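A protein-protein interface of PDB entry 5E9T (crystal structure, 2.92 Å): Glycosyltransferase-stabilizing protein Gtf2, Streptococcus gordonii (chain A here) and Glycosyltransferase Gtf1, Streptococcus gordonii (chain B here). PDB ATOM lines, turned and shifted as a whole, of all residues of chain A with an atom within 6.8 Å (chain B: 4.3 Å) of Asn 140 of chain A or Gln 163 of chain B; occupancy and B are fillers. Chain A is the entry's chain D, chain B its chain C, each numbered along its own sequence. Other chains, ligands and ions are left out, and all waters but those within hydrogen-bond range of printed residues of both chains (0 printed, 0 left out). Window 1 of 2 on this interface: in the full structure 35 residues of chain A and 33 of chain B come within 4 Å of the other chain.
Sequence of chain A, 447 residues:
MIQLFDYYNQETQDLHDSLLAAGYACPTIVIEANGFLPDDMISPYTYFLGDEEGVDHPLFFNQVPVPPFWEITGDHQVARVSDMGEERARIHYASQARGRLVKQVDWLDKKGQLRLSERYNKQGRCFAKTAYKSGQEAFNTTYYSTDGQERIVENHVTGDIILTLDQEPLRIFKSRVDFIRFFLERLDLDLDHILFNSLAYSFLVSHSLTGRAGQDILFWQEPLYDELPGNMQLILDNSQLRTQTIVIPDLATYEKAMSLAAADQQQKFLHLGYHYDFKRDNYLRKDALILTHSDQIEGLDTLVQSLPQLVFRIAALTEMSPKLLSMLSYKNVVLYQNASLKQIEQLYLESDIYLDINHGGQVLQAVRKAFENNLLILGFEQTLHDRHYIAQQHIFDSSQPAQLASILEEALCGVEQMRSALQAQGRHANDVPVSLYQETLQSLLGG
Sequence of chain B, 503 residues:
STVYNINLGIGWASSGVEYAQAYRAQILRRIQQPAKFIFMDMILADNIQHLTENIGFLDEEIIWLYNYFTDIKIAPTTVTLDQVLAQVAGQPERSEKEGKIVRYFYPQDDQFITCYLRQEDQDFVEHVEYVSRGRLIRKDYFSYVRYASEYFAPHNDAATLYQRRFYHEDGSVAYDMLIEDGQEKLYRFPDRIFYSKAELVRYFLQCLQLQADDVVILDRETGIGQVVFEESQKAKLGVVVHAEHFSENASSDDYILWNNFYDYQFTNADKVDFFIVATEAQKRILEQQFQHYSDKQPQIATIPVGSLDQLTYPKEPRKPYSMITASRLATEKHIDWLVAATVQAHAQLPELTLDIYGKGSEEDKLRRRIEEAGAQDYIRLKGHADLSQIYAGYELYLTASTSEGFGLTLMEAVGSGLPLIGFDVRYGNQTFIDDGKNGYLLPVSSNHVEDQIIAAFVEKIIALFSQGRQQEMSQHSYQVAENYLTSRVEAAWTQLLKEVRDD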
ATOM      1  N   LEU A 116      24.868 -20.796  32.477  1.00  0.00           N
ATOM      2  CA  LEU A 116      24.981 -20.866  31.029  1.00  0.00           C
ATOM      3  C   LEU A 116      24.550 -22.235  30.521  1.00  0.00           C
ATOM      4  O   LEU A 116      24.690 -23.248  31.212  1.00  0.00           O
ATOM      5  CB  LEU A 116      26.414 -20.610  30.558  1.00  0.00           C
ATOM      6  CG  LEU A 116      27.279 -19.585  31.279  1.00  0.00           C
ATOM      7  CD1 LEU A 116      28.603 -19.461  30.545  1.00  0.00           C
ATOM      8  CD2 LEU A 116      26.578 -18.237  31.381  1.00  0.00           C
ATOM      9  N   LYS A 129      25.399 -19.802  23.214  1.00  0.00           N
ATOM     10  CA  LYS A 129      25.398 -19.740  24.667  1.00  0.00           C
ATOM     11  C   LYS A 129      24.081 -19.121  25.107  1.00  0.00           C
ATOM     12  O   LYS A 129      23.714 -18.039  24.635  1.00  0.00           O
ATOM     13  CB  LYS A 129      26.569 -18.912  25.210  1.00  0.00           C
ATOM     14  CG  LYS A 129      27.964 -19.415  24.865  1.00  0.00           C
ATOM     15  CD  LYS A 129      28.979 -18.854  25.864  1.00  0.00           C
ATOM     16  CE  LYS A 129      30.400 -18.837  25.314  1.00  0.00           C
ATOM     17  NZ  LYS A 129      31.073 -17.533  25.596  1.00  0.00           N
ATOM     18  N   THR A 130      23.368 -19.808  25.991  1.00  0.00           N
ATOM     19  CA  THR A 130      22.182 -19.252  26.625  1.00  0.00           C
ATOM     20  C   THR A 130      22.540 -18.811  28.037  1.00  0.00           C
ATOM     21  O   THR A 130      23.138 -19.578  28.799  1.00  0.00           O
ATOM     22  CB  THR A 130      21.038 -20.266  26.659  1.00  0.00           C
ATOM     23  OG1 THR A 130      20.596 -20.528  25.323  1.00  0.00           O
ATOM     24  CG2 THR A 130      19.871 -19.725  27.468  1.00  0.00           C
ATOM     25  N   ALA A 131      22.191 -17.575  28.377  1.00  0.00           N
ATOM     26  CA  ALA A 131      22.444 -17.026  29.700  1.00  0.00           C
ATOM     27  C   ALA A 131      21.154 -17.020  30.508  1.00  0.00           C
ATOM     28  O   ALA A 131      20.074 -16.759  29.970  1.00  0.00           O
ATOM     29  CB  ALA A 131      23.018 -15.612  29.605  1.00  0.00           C
ATOM     30  N   TYR A 132      21.271 -17.312  31.801  1.00  0.00           N
ATOM     31  CA  TYR A 132      20.122 -17.445  32.684  1.00  0.00           C
ATOM     32  C   TYR A 132      20.147 -16.371  33.763  1.00  0.00           C
ATOM     33  O   TYR A 132      21.214 -15.916  34.188  1.00  0.00           O
ATOM     34  CB  TYR A 132      20.084 -18.831  33.341  1.00  0.00           C
ATOM     35  CG  TYR A 132      19.746 -19.955  32.387  1.00  0.00           C
ATOM     36  CD1 TYR A 132      20.717 -20.512  31.564  1.00  0.00           C
ATOM     37  CD2 TYR A 132      18.456 -20.462  32.313  1.00  0.00           C
ATOM     38  CE1 TYR A 132      20.412 -21.538  30.692  1.00  0.00           C
ATOM     39  CE2 TYR A 132      18.141 -21.490  31.443  1.00  0.00           C
ATOM     40  CZ  TYR A 132      19.124 -22.023  30.636  1.00  0.00           C
ATOM     41  OH  TYR A 132      18.814 -23.046  29.770  1.00  0.00           O
ATOM     42  N   LYS A 133      18.956 -15.968  34.198  1.00  0.00           N
ATOM     43  CA  LYS A 133      18.801 -15.043  35.306  1.00  0.00           C
ATOM     44  C   LYS A 133      18.352 -15.809  36.553  1.00  0.00           C
ATOM     45  O   LYS A 133      18.279 -17.040  36.557  1.00  0.00           O
ATOM     46  CB  LYS A 133      17.855 -13.901  34.927  1.00  0.00           C
ATOM     47  CG  LYS A 133      16.425 -14.292  34.622  1.00  0.00           C
ATOM     48  CD  LYS A 133      15.646 -13.067  34.164  1.00  0.00           C
ATOM     49  CE  LYS A 133      14.196 -13.392  33.855  1.00  0.00           C
ATOM     50  NZ  LYS A 133      13.321 -12.199  34.039  1.00  0.00           N
ATOM     51  N   GLU A 137      15.603 -18.921  35.017  1.00  0.00           N
ATOM     52  CA  GLU A 137      14.827 -18.555  33.846  1.00  0.00           C
ATOM     53  C   GLU A 137      15.780 -18.072  32.762  1.00  0.00           C
ATOM     54  O   GLU A 137      16.740 -17.349  33.043  1.00  0.00           O
ATOM     55  CB  GLU A 137      13.814 -17.458  34.178  1.00  0.00           C
ATOM     56  CG  GLU A 137      13.011 -17.715  35.443  1.00  0.00           C
ATOM     57  CD  GLU A 137      11.768 -16.841  35.527  1.00  0.00           C
ATOM     58  OE1 GLU A 137      10.832 -17.202  36.258  1.00  0.00           O
ATOM     59  OE2 GLU A 137      11.731 -15.791  34.863  1.00  0.00           O
ATOM     60  N   ALA A 138      15.516 -18.485  31.526  1.00  0.00           N
ATOM     61  CA  ALA A 138      16.385 -18.119  30.418  1.00  0.00           C
ATOM     62  C   ALA A 138      16.301 -16.624  30.136  1.00  0.00           C
ATOM     63  O   ALA A 138      15.215 -16.038  30.115  1.00  0.00           O
ATOM     64  CB  ALA A 138      16.009 -18.914  29.168  1.00  0.00           C
ATOM     65  N   PHE A 139      17.463 -16.006  29.916  1.00  0.00           N
ATOM     66  CA  PHE A 139      17.516 -14.580  29.615  1.00  0.00           C
ATOM     67  C   PHE A 139      17.699 -14.336  28.122  1.00  0.00           C
ATOM     68  O   PHE A 139      16.764 -13.895  27.447  1.00  0.00           O
ATOM     69  CB  PHE A 139      18.636 -13.898  30.402  1.00  0.00           C
ATOM     70  CG  PHE A 139      18.960 -12.521  29.910  1.00  0.00           C
ATOM     71  CD1 PHE A 139      18.022 -11.506  29.988  1.00  0.00           C
ATOM     72  CD2 PHE A 139      20.199 -12.243  29.359  1.00  0.00           C
ATOM     73  CE1 PHE A 139      18.313 -10.237  29.525  1.00  0.00           C
ATOM     74  CE2 PHE A 139      20.498 -10.976  28.899  1.00  0.00           C
ATOM     75  CZ  PHE A 139      19.553  -9.970  28.982  1.00  0.00           C
ATOM     76  N   ASN A 140      18.892 -14.605  27.589  1.00  0.00           N
ATOM     77  CA  ASN A 140      19.127 -14.439  26.162  1.00  0.00           C
ATOM     78  C   ASN A 140      19.892 -15.640  25.626  1.00  0.00           C
ATOM     79  O   ASN A 140      20.395 -16.476  26.382  1.00  0.00           O
ATOM     80  CB  ASN A 140      19.845 -13.107  25.842  1.00  0.00           C
ATOM     81  CG  ASN A 140      21.364 -13.138  26.072  1.00  0.00           C
ATOM     82  OD1 ASN A 140      21.966 -14.160  26.401  1.00  0.00           O
ATOM     83  ND2 ASN A 140      21.990 -11.983  25.874  1.00  0.00           N
ATOM     84  N   THR A 141      19.962 -15.724  24.301  1.00  0.00           N
ATOM     85  CA  THR A 141      20.799 -16.699  23.619  1.00  0.00           C
ATOM     86  C   THR A 141      21.575 -15.991  22.520  1.00  0.00           C
ATOM     87  O   THR A 141      20.979 -15.328  21.666  1.00  0.00           O
ATOM     88  CB  THR A 141      19.978 -17.842  23.019  1.00  0.00           C
ATOM     89  OG1 THR A 141      19.175 -18.449  24.039  1.00  0.00           O
ATOM     90  CG2 THR A 141      20.901 -18.891  22.422  1.00  0.00           C
ATOM     91  N   THR A 142      22.896 -16.123  22.550  1.00  0.00           N
ATOM     92  CA  THR A 142      23.755 -15.598  21.500  1.00  0.00           C
ATOM     93  C   THR A 142      24.168 -16.740  20.584  1.00  0.00           C
ATOM     94  O   THR A 142      24.623 -17.786  21.056  1.00  0.00           O
ATOM     95  CB  THR A 142      24.997 -14.917  22.077  1.00  0.00           C
ATOM     96  OG1 THR A 142      24.602 -13.910  23.017  1.00  0.00           O
ATOM     97  CG2 THR A 142      25.805 -14.267  20.965  1.00  0.00           C
ATOM     98  N   TYR A 144      26.733 -17.608  17.429  1.00  0.00           N
ATOM     99  CA  TYR A 144      28.018 -17.068  17.003  1.00  0.00           C
ATOM    100  C   TYR A 144      28.441 -17.619  15.653  1.00  0.00           C
ATOM    101  O   TYR A 144      28.302 -18.816  15.391  1.00  0.00           O
ATOM    102  CB  TYR A 144      29.124 -17.400  18.006  1.00  0.00           C
ATOM    103  CG  TYR A 144      28.895 -16.907  19.405  1.00  0.00           C
ATOM    104  CD1 TYR A 144      28.146 -17.647  20.307  1.00  0.00           C
ATOM    105  CD2 TYR A 144      29.452 -15.713  19.835  1.00  0.00           C
ATOM    106  CE1 TYR A 144      27.944 -17.204  21.593  1.00  0.00           C
ATOM    107  CE2 TYR A 144      29.257 -15.263  21.117  1.00  0.00           C
ATOM    108  CZ  TYR A 144      28.504 -16.012  21.995  1.00  0.00           C
ATOM    109  OH  TYR A 144      28.306 -15.563  23.281  1.00  0.00           O
ATOM    110  N   VAL A 153      21.274 -12.552  18.548  1.00  0.00           N
ATOM    111  CA  VAL A 153      21.078 -12.476  19.991  1.00  0.00           C
ATOM    112  C   VAL A 153      19.579 -12.346  20.217  1.00  0.00           C
ATOM    113  O   VAL A 153      18.998 -11.288  19.949  1.00  0.00           O
ATOM    114  CB  VAL A 153      21.824 -11.296  20.625  1.00  0.00           C
ATOM    115  CG1 VAL A 153      21.666 -11.322  22.140  1.00  0.00           C
ATOM    116  CG2 VAL A 153      23.291 -11.311  20.221  1.00  0.00           C
ATOM    117  N   GLU A 154      18.960 -13.396  20.745  1.00  0.00           N
ATOM    118  CA  GLU A 154      17.526 -13.398  20.991  1.00  0.00           C
ATOM    119  C   GLU A 154      17.273 -13.099  22.460  1.00  0.00           C
ATOM    120  O   GLU A 154      17.890 -13.709  23.340  1.00  0.00           O
ATOM    121  CB  GLU A 154      16.882 -14.731  20.609  1.00  0.00           C
ATOM    122  CG  GLU A 154      15.399 -14.790  20.965  1.00  0.00           C
ATOM    123  CD  GLU A 154      14.632 -15.837  20.181  1.00  0.00           C
ATOM    124  OE1 GLU A 154      15.231 -16.474  19.289  1.00  0.00           O
ATOM    125  OE2 GLU A 154      13.426 -16.019  20.457  1.00  0.00           O
ATOM    126  N   ASN A 155      16.376 -12.157  22.716  1.00  0.00           N
ATOM    127  CA  ASN A 155      15.967 -11.823  24.072  1.00  0.00           C
ATOM    128  C   ASN A 155      14.751 -12.669  24.422  1.00  0.00           C
ATOM    129  O   ASN A 155      13.728 -12.601  23.736  1.00  0.00           O
ATOM    130  CB  ASN A 155      15.646 -10.334  24.183  1.00  0.00           C
ATOM    131  CG  ASN A 155      15.624  -9.848  25.614  1.00  0.00           C
ATOM    132  OD1 ASN A 155      14.645 -10.047  26.337  1.00  0.00           O
ATOM    133  ND2 ASN A 155      16.705  -9.199  26.032  1.00  0.00           N
ATOM    134  N   HIS A 156      14.863 -13.477  25.470  1.00  0.00           N
ATOM    135  CA  HIS A 156      13.764 -14.362  25.823  1.00  0.00           C
ATOM    136  C   HIS A 156      12.720 -13.694  26.706  1.00  0.00           C
ATOM    137  O   HIS A 156      11.653 -14.276  26.922  1.00  0.00           O
ATOM    138  CB  HIS A 156      14.302 -15.627  26.500  1.00  0.00           C
ATOM    139  CG  HIS A 156      15.246 -16.409  25.639  1.00  0.00           C
ATOM    140  ND1 HIS A 156      14.827 -17.137  24.548  1.00  0.00           N
ATOM    141  CD2 HIS A 156      16.589 -16.564  25.701  1.00  0.00           C
ATOM    142  CE1 HIS A 156      15.870 -17.712  23.977  1.00  0.00           C
ATOM    143  NE2 HIS A 156      16.952 -17.379  24.656  1.00  0.00           N
ATOM    144  N   VAL A 157      13.009 -12.514  27.253  1.00  0.00           N
ATOM    145  CA  VAL A 157      11.975 -11.758  27.954  1.00  0.00           C
ATOM    146  C   VAL A 157      11.145 -10.927  26.980  1.00  0.00           C
ATOM    147  O   VAL A 157       9.913 -10.901  27.064  1.00  0.00           O
ATOM    148  CB  VAL A 157      12.606 -10.884  29.049  1.00  0.00           C
ATOM    149  CG1 VAL A 157      11.527 -10.162  29.844  1.00  0.00           C
ATOM    150  CG2 VAL A 157      13.475 -11.733  29.966  1.00  0.00           C
ATOM    151  N   GLU B 150      25.982  -4.039  26.293  1.00  0.00           N
ATOM    152  CA  GLU B 150      25.168  -4.441  27.429  1.00  0.00           C
ATOM    153  C   GLU B 150      23.828  -4.935  26.911  1.00  0.00           C
ATOM    154  O   GLU B 150      23.273  -4.367  25.967  1.00  0.00           O
ATOM    155  CB  GLU B 150      24.951  -3.274  28.414  1.00  0.00           C
ATOM    156  CG  GLU B 150      26.198  -2.804  29.156  1.00  0.00           C
ATOM    157  CD  GLU B 150      25.925  -1.616  30.082  1.00  0.00           C
ATOM    158  OE1 GLU B 150      24.785  -1.123  30.116  1.00  0.00           O
ATOM    159  OE2 GLU B 150      26.853  -1.171  30.779  1.00  0.00           O
ATOM    160  N   TYR B 151      23.309  -5.992  27.525  1.00  0.00           N
ATOM    161  CA  TYR B 151      22.004  -6.529  27.171  1.00  0.00           C
ATOM    162  C   TYR B 151      21.065  -6.404  28.361  1.00  0.00           C
ATOM    163  O   TYR B 151      21.473  -6.602  29.511  1.00  0.00           O
ATOM    164  CB  TYR B 151      22.112  -7.981  26.700  1.00  0.00           C
ATOM    165  CG  TYR B 151      22.829  -8.092  25.374  1.00  0.00           C
ATOM    166  CD1 TYR B 151      24.202  -8.302  25.320  1.00  0.00           C
ATOM    167  CD2 TYR B 151      22.140  -7.953  24.176  1.00  0.00           C
ATOM    168  CE1 TYR B 151      24.865  -8.392  24.111  1.00  0.00           C
ATOM    169  CE2 TYR B 151      22.793  -8.039  22.962  1.00  0.00           C
ATOM    170  CZ  TYR B 151      24.157  -8.261  22.936  1.00  0.00           C
ATOM    171  OH  TYR B 151      24.821  -8.350  21.732  1.00  0.00           O
ATOM    172  N   LEU B 161      19.993  -4.578  33.902  1.00  0.00           N
ATOM    173  CA  LEU B 161      21.213  -5.081  33.281  1.00  0.00           C
ATOM    174  C   LEU B 161      21.407  -6.545  33.656  1.00  0.00           C
ATOM    175  O   LEU B 161      21.551  -6.864  34.839  1.00  0.00           O
ATOM    176  CB  LEU B 161      22.400  -4.247  33.759  1.00  0.00           C
ATOM    177  CG  LEU B 161      23.809  -4.572  33.288  1.00  0.00           C
ATOM    178  CD1 LEU B 161      23.820  -4.811  31.795  1.00  0.00           C
ATOM    179  CD2 LEU B 161      24.770  -3.451  33.670  1.00  0.00           C
ATOM    180  N   TYR B 162      21.330  -7.451  32.673  1.00  0.00           N
ATOM    181  CA  TYR B 162      21.677  -8.843  32.934  1.00  0.00           C
ATOM    182  C   TYR B 162      23.015  -9.325  32.380  1.00  0.00           C
ATOM    183  O   TYR B 162      23.531 -10.328  32.883  1.00  0.00           O
ATOM    184  CB  TYR B 162      20.576  -9.764  32.399  1.00  0.00           C
ATOM    185  CG  TYR B 162      19.293  -9.631  33.174  1.00  0.00           C
ATOM    186  CD1 TYR B 162      19.184 -10.148  34.456  1.00  0.00           C
ATOM    187  CD2 TYR B 162      18.194  -8.979  32.634  1.00  0.00           C
ATOM    188  CE1 TYR B 162      18.014 -10.029  35.173  1.00  0.00           C
ATOM    189  CE2 TYR B 162      17.019  -8.855  33.344  1.00  0.00           C
ATOM    190  CZ  TYR B 162      16.934  -9.382  34.613  1.00  0.00           C
ATOM    191  OH  TYR B 162      15.764  -9.260  35.325  1.00  0.00           O
ATOM    192  N   GLN B 163      23.605  -8.651  31.391  1.00  0.00           N
ATOM    193  CA  GLN B 163      24.803  -9.205  30.766  1.00  0.00           C
ATOM    194  C   GLN B 163      25.621  -8.089  30.135  1.00  0.00           C
ATOM    195  O   GLN B 163      25.068  -7.125  29.600  1.00  0.00           O
ATOM    196  CB  GLN B 163      24.449 -10.268  29.712  1.00  0.00           C
ATOM    197  CG  GLN B 163      25.657 -10.960  29.072  1.00  0.00           C
ATOM    198  CD  GLN B 163      25.267 -12.107  28.146  1.00  0.00           C
ATOM    199  OE1 GLN B 163      26.126 -12.822  27.625  1.00  0.00           O
ATOM    200  NE2 GLN B 163      23.968 -12.287  27.943  1.00  0.00           N
ATOM    201  N   ARG B 164      26.945  -8.251  30.171  1.00  0.00           N
ATOM    202  CA  ARG B 164      27.864  -7.296  29.562  1.00  0.00           C
ATOM    203  C   ARG B 164      28.952  -8.065  28.830  1.00  0.00           C
ATOM    204  O   ARG B 164      29.677  -8.854  29.443  1.00  0.00           O
ATOM    205  CB  ARG B 164      28.466  -6.358  30.614  1.00  0.00           C
ATOM    206  CG  ARG B 164      29.623  -5.525  30.107  1.00  0.00           C
ATOM    207  CD  ARG B 164      29.654  -4.141  30.747  1.00  0.00           C
ATOM    208  NE  ARG B 164      29.909  -4.177  32.185  1.00  0.00           N
ATOM    209  CZ  ARG B 164      29.031  -3.807  33.113  1.00  0.00           C
ATOM    210  NH1 ARG B 164      27.832  -3.365  32.758  1.00  0.00           N
ATOM    211  NH2 ARG B 164      29.354  -3.872  34.398  1.00  0.00           N
ATOM    212  N   ARG B 165      29.067  -7.834  27.525  1.00  0.00           N
ATOM    213  CA  ARG B 165      29.990  -8.565  26.668  1.00  0.00           C
ATOM    214  C   ARG B 165      31.091  -7.638  26.170  1.00  0.00           C
ATOM    215  O   ARG B 165      30.861  -6.451  25.930  1.00  0.00           O
ATOM    216  CB  ARG B 165      29.241  -9.189  25.485  1.00  0.00           C
ATOM    217  CG  ARG B 165      29.968 -10.336  24.815  1.00  0.00           C
ATOM    218  CD  ARG B 165      29.093 -11.027  23.775  1.00  0.00           C
ATOM    219  NE  ARG B 165      28.309 -12.125  24.333  1.00  0.00           N
ATOM    220  CZ  ARG B 165      26.983 -12.214  24.262  1.00  0.00           C
ATOM    221  NH1 ARG B 165      26.284 -11.270  23.646  1.00  0.00           N
ATOM    222  NH2 ARG B 165      26.356 -13.252  24.799  1.00  0.00           N
ATOM    223  N   ASP B 176      32.479 -12.477  28.504  1.00  0.00           N
ATOM    224  CA  ASP B 176      31.312 -11.735  28.963  1.00  0.00           C
ATOM    225  C   ASP B 176      31.045 -12.061  30.428  1.00  0.00           C
ATOM    226  O   ASP B 176      31.709 -12.910  31.032  1.00  0.00           O
ATOM    227  CB  ASP B 176      30.090 -12.019  28.080  1.00  0.00           C
ATOM    228  CG  ASP B 176      29.743 -13.496  28.004  1.00  0.00           C
ATOM    229  OD1 ASP B 176      29.544 -14.127  29.064  1.00  0.00           O
ATOM    230  OD2 ASP B 176      29.662 -14.027  26.875  1.00  0.00           O
ATOM    231  N   MET B 177      30.042 -11.390  30.989  1.00  0.00           N
ATOM    232  CA  MET B 177      29.752 -11.478  32.414  1.00  0.00           C
ATOM    233  C   MET B 177      28.257 -11.402  32.707  1.00  0.00           C
ATOM    234  O   MET B 177      27.493 -10.813  31.944  1.00  0.00           O
ATOM    235  CB  MET B 177      30.487 -10.367  33.171  1.00  0.00           C
ATOM    236  CG  MET B 177      30.036  -8.956  32.818  1.00  0.00           C
ATOM    237  SD  MET B 177      31.185  -7.578  33.586  1.00  0.00           S
ATOM    238  CE  MET B 177      32.839  -8.048  32.673  1.00  0.00           C
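Ala 131 of chain A touches Gln 163 of chain B (CB to NE2, 3.8 Å).
CB of Lys 133 of chain A touches CE1 of Tyr 162 of chain B, 3.9 Å away.
O of Tyr 151 of chain B touches CZ of Phe 139 of chain A (3.9 Å).
CD2 of Tyr 162 of chain B touches CE1 of Phe 139 of chain A, 3.4 Å away.
NE2 of Gln 163 of chain B touches CE2 of Phe 139 of chain A, at 3.8 Å.
Val 153 of chain A touches Tyr 151 of chain B (CG1 to CE2, 3.6 Å).
O of Tyr 151 of chain B lies within hydrogen-bond range of N of Tyr 162 of chain B (3.3 Å).
The backbone carbonyl oxygen of Gln 163 of chain B is in hydrogen-bond range of the backbone NH of Tyr 151 of chain B (2.9 Å).
OD2 of Asp 176 of chain B lies within salt-bridge range of NE of Arg 165 of chain B (3.5 Å).
The backbone NH (N) of Phe 139 of chain A is in hydrogen-bond range of the backbone carbonyl oxygen (O) of Ala 131 of chain A, 2.7 Å away.
The backbone NH (N) of Ala 131 of chain A is in hydrogen-bond range of the backbone carbonyl oxygen (O) of Asn 140 of chain A (2.9 Å).
O of Phe 139 of chain A is in hydrogen-bond range of N of His 156 of chain A (2.8 Å).
The side-chain amide nitrogen (NE2) of Gln 163 of chain B lies close to the side-chain amide nitrogen (ND2) of Asn 140 of chain A, at 2.9 Å.
NH2 of Arg 165 of chain B is in hydrogen-bond range of OG1 of Thr 142 of chain A, at 2.6 Å.
OH of Tyr 144 of chain A lies within hydrogen-bond range of NH2 of Arg 165 of chain B.
The side-chain carboxylate (OD2) of Asp 176 of chain B lies within salt-bridge range of the side-chain amino group (NZ) of Lys 129 of chain A (3.99 Å).
Of the 9 printed residues of chain B, 5 touch a printed residue of chain A.
Hydrophobic or aromatic side chains of chain B that line the printed part of chain A: Tyr 151 and Tyr 162.
Along chain B the printed residues that touch a printed residue of chain A span positions 151 to 176.
Among the printed residues, 10 pairs touch across the chains.
Leu 116 of chain A touches none of the printed residues of chain B.
Thr 130 of chain A touches none of the printed residues of chain B.
Of the printed residues of chain B, Ala 131 of chain A touches Gln 163.
Of the printed residues of chain B, Asn 140 of chain A touches Gln 163.
Of the printed residues of chain A, Tyr 151 of chain B touches Phe 139 (3.9 Å) and Val 153 (3.6 Å).
Of chain A, only Ala 131, Phe 139 and Asn 140 come within 4 Å of Gln 163 of chain B.
The nearest printed residue of chain B that does not touch Asn 140 of chain A is Tyr 151 of chain B (4.01 Å).
The nearest residue of chain A that does not touch Gln 163 of chain B is Thr 142 of chain A (5.0 Å).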
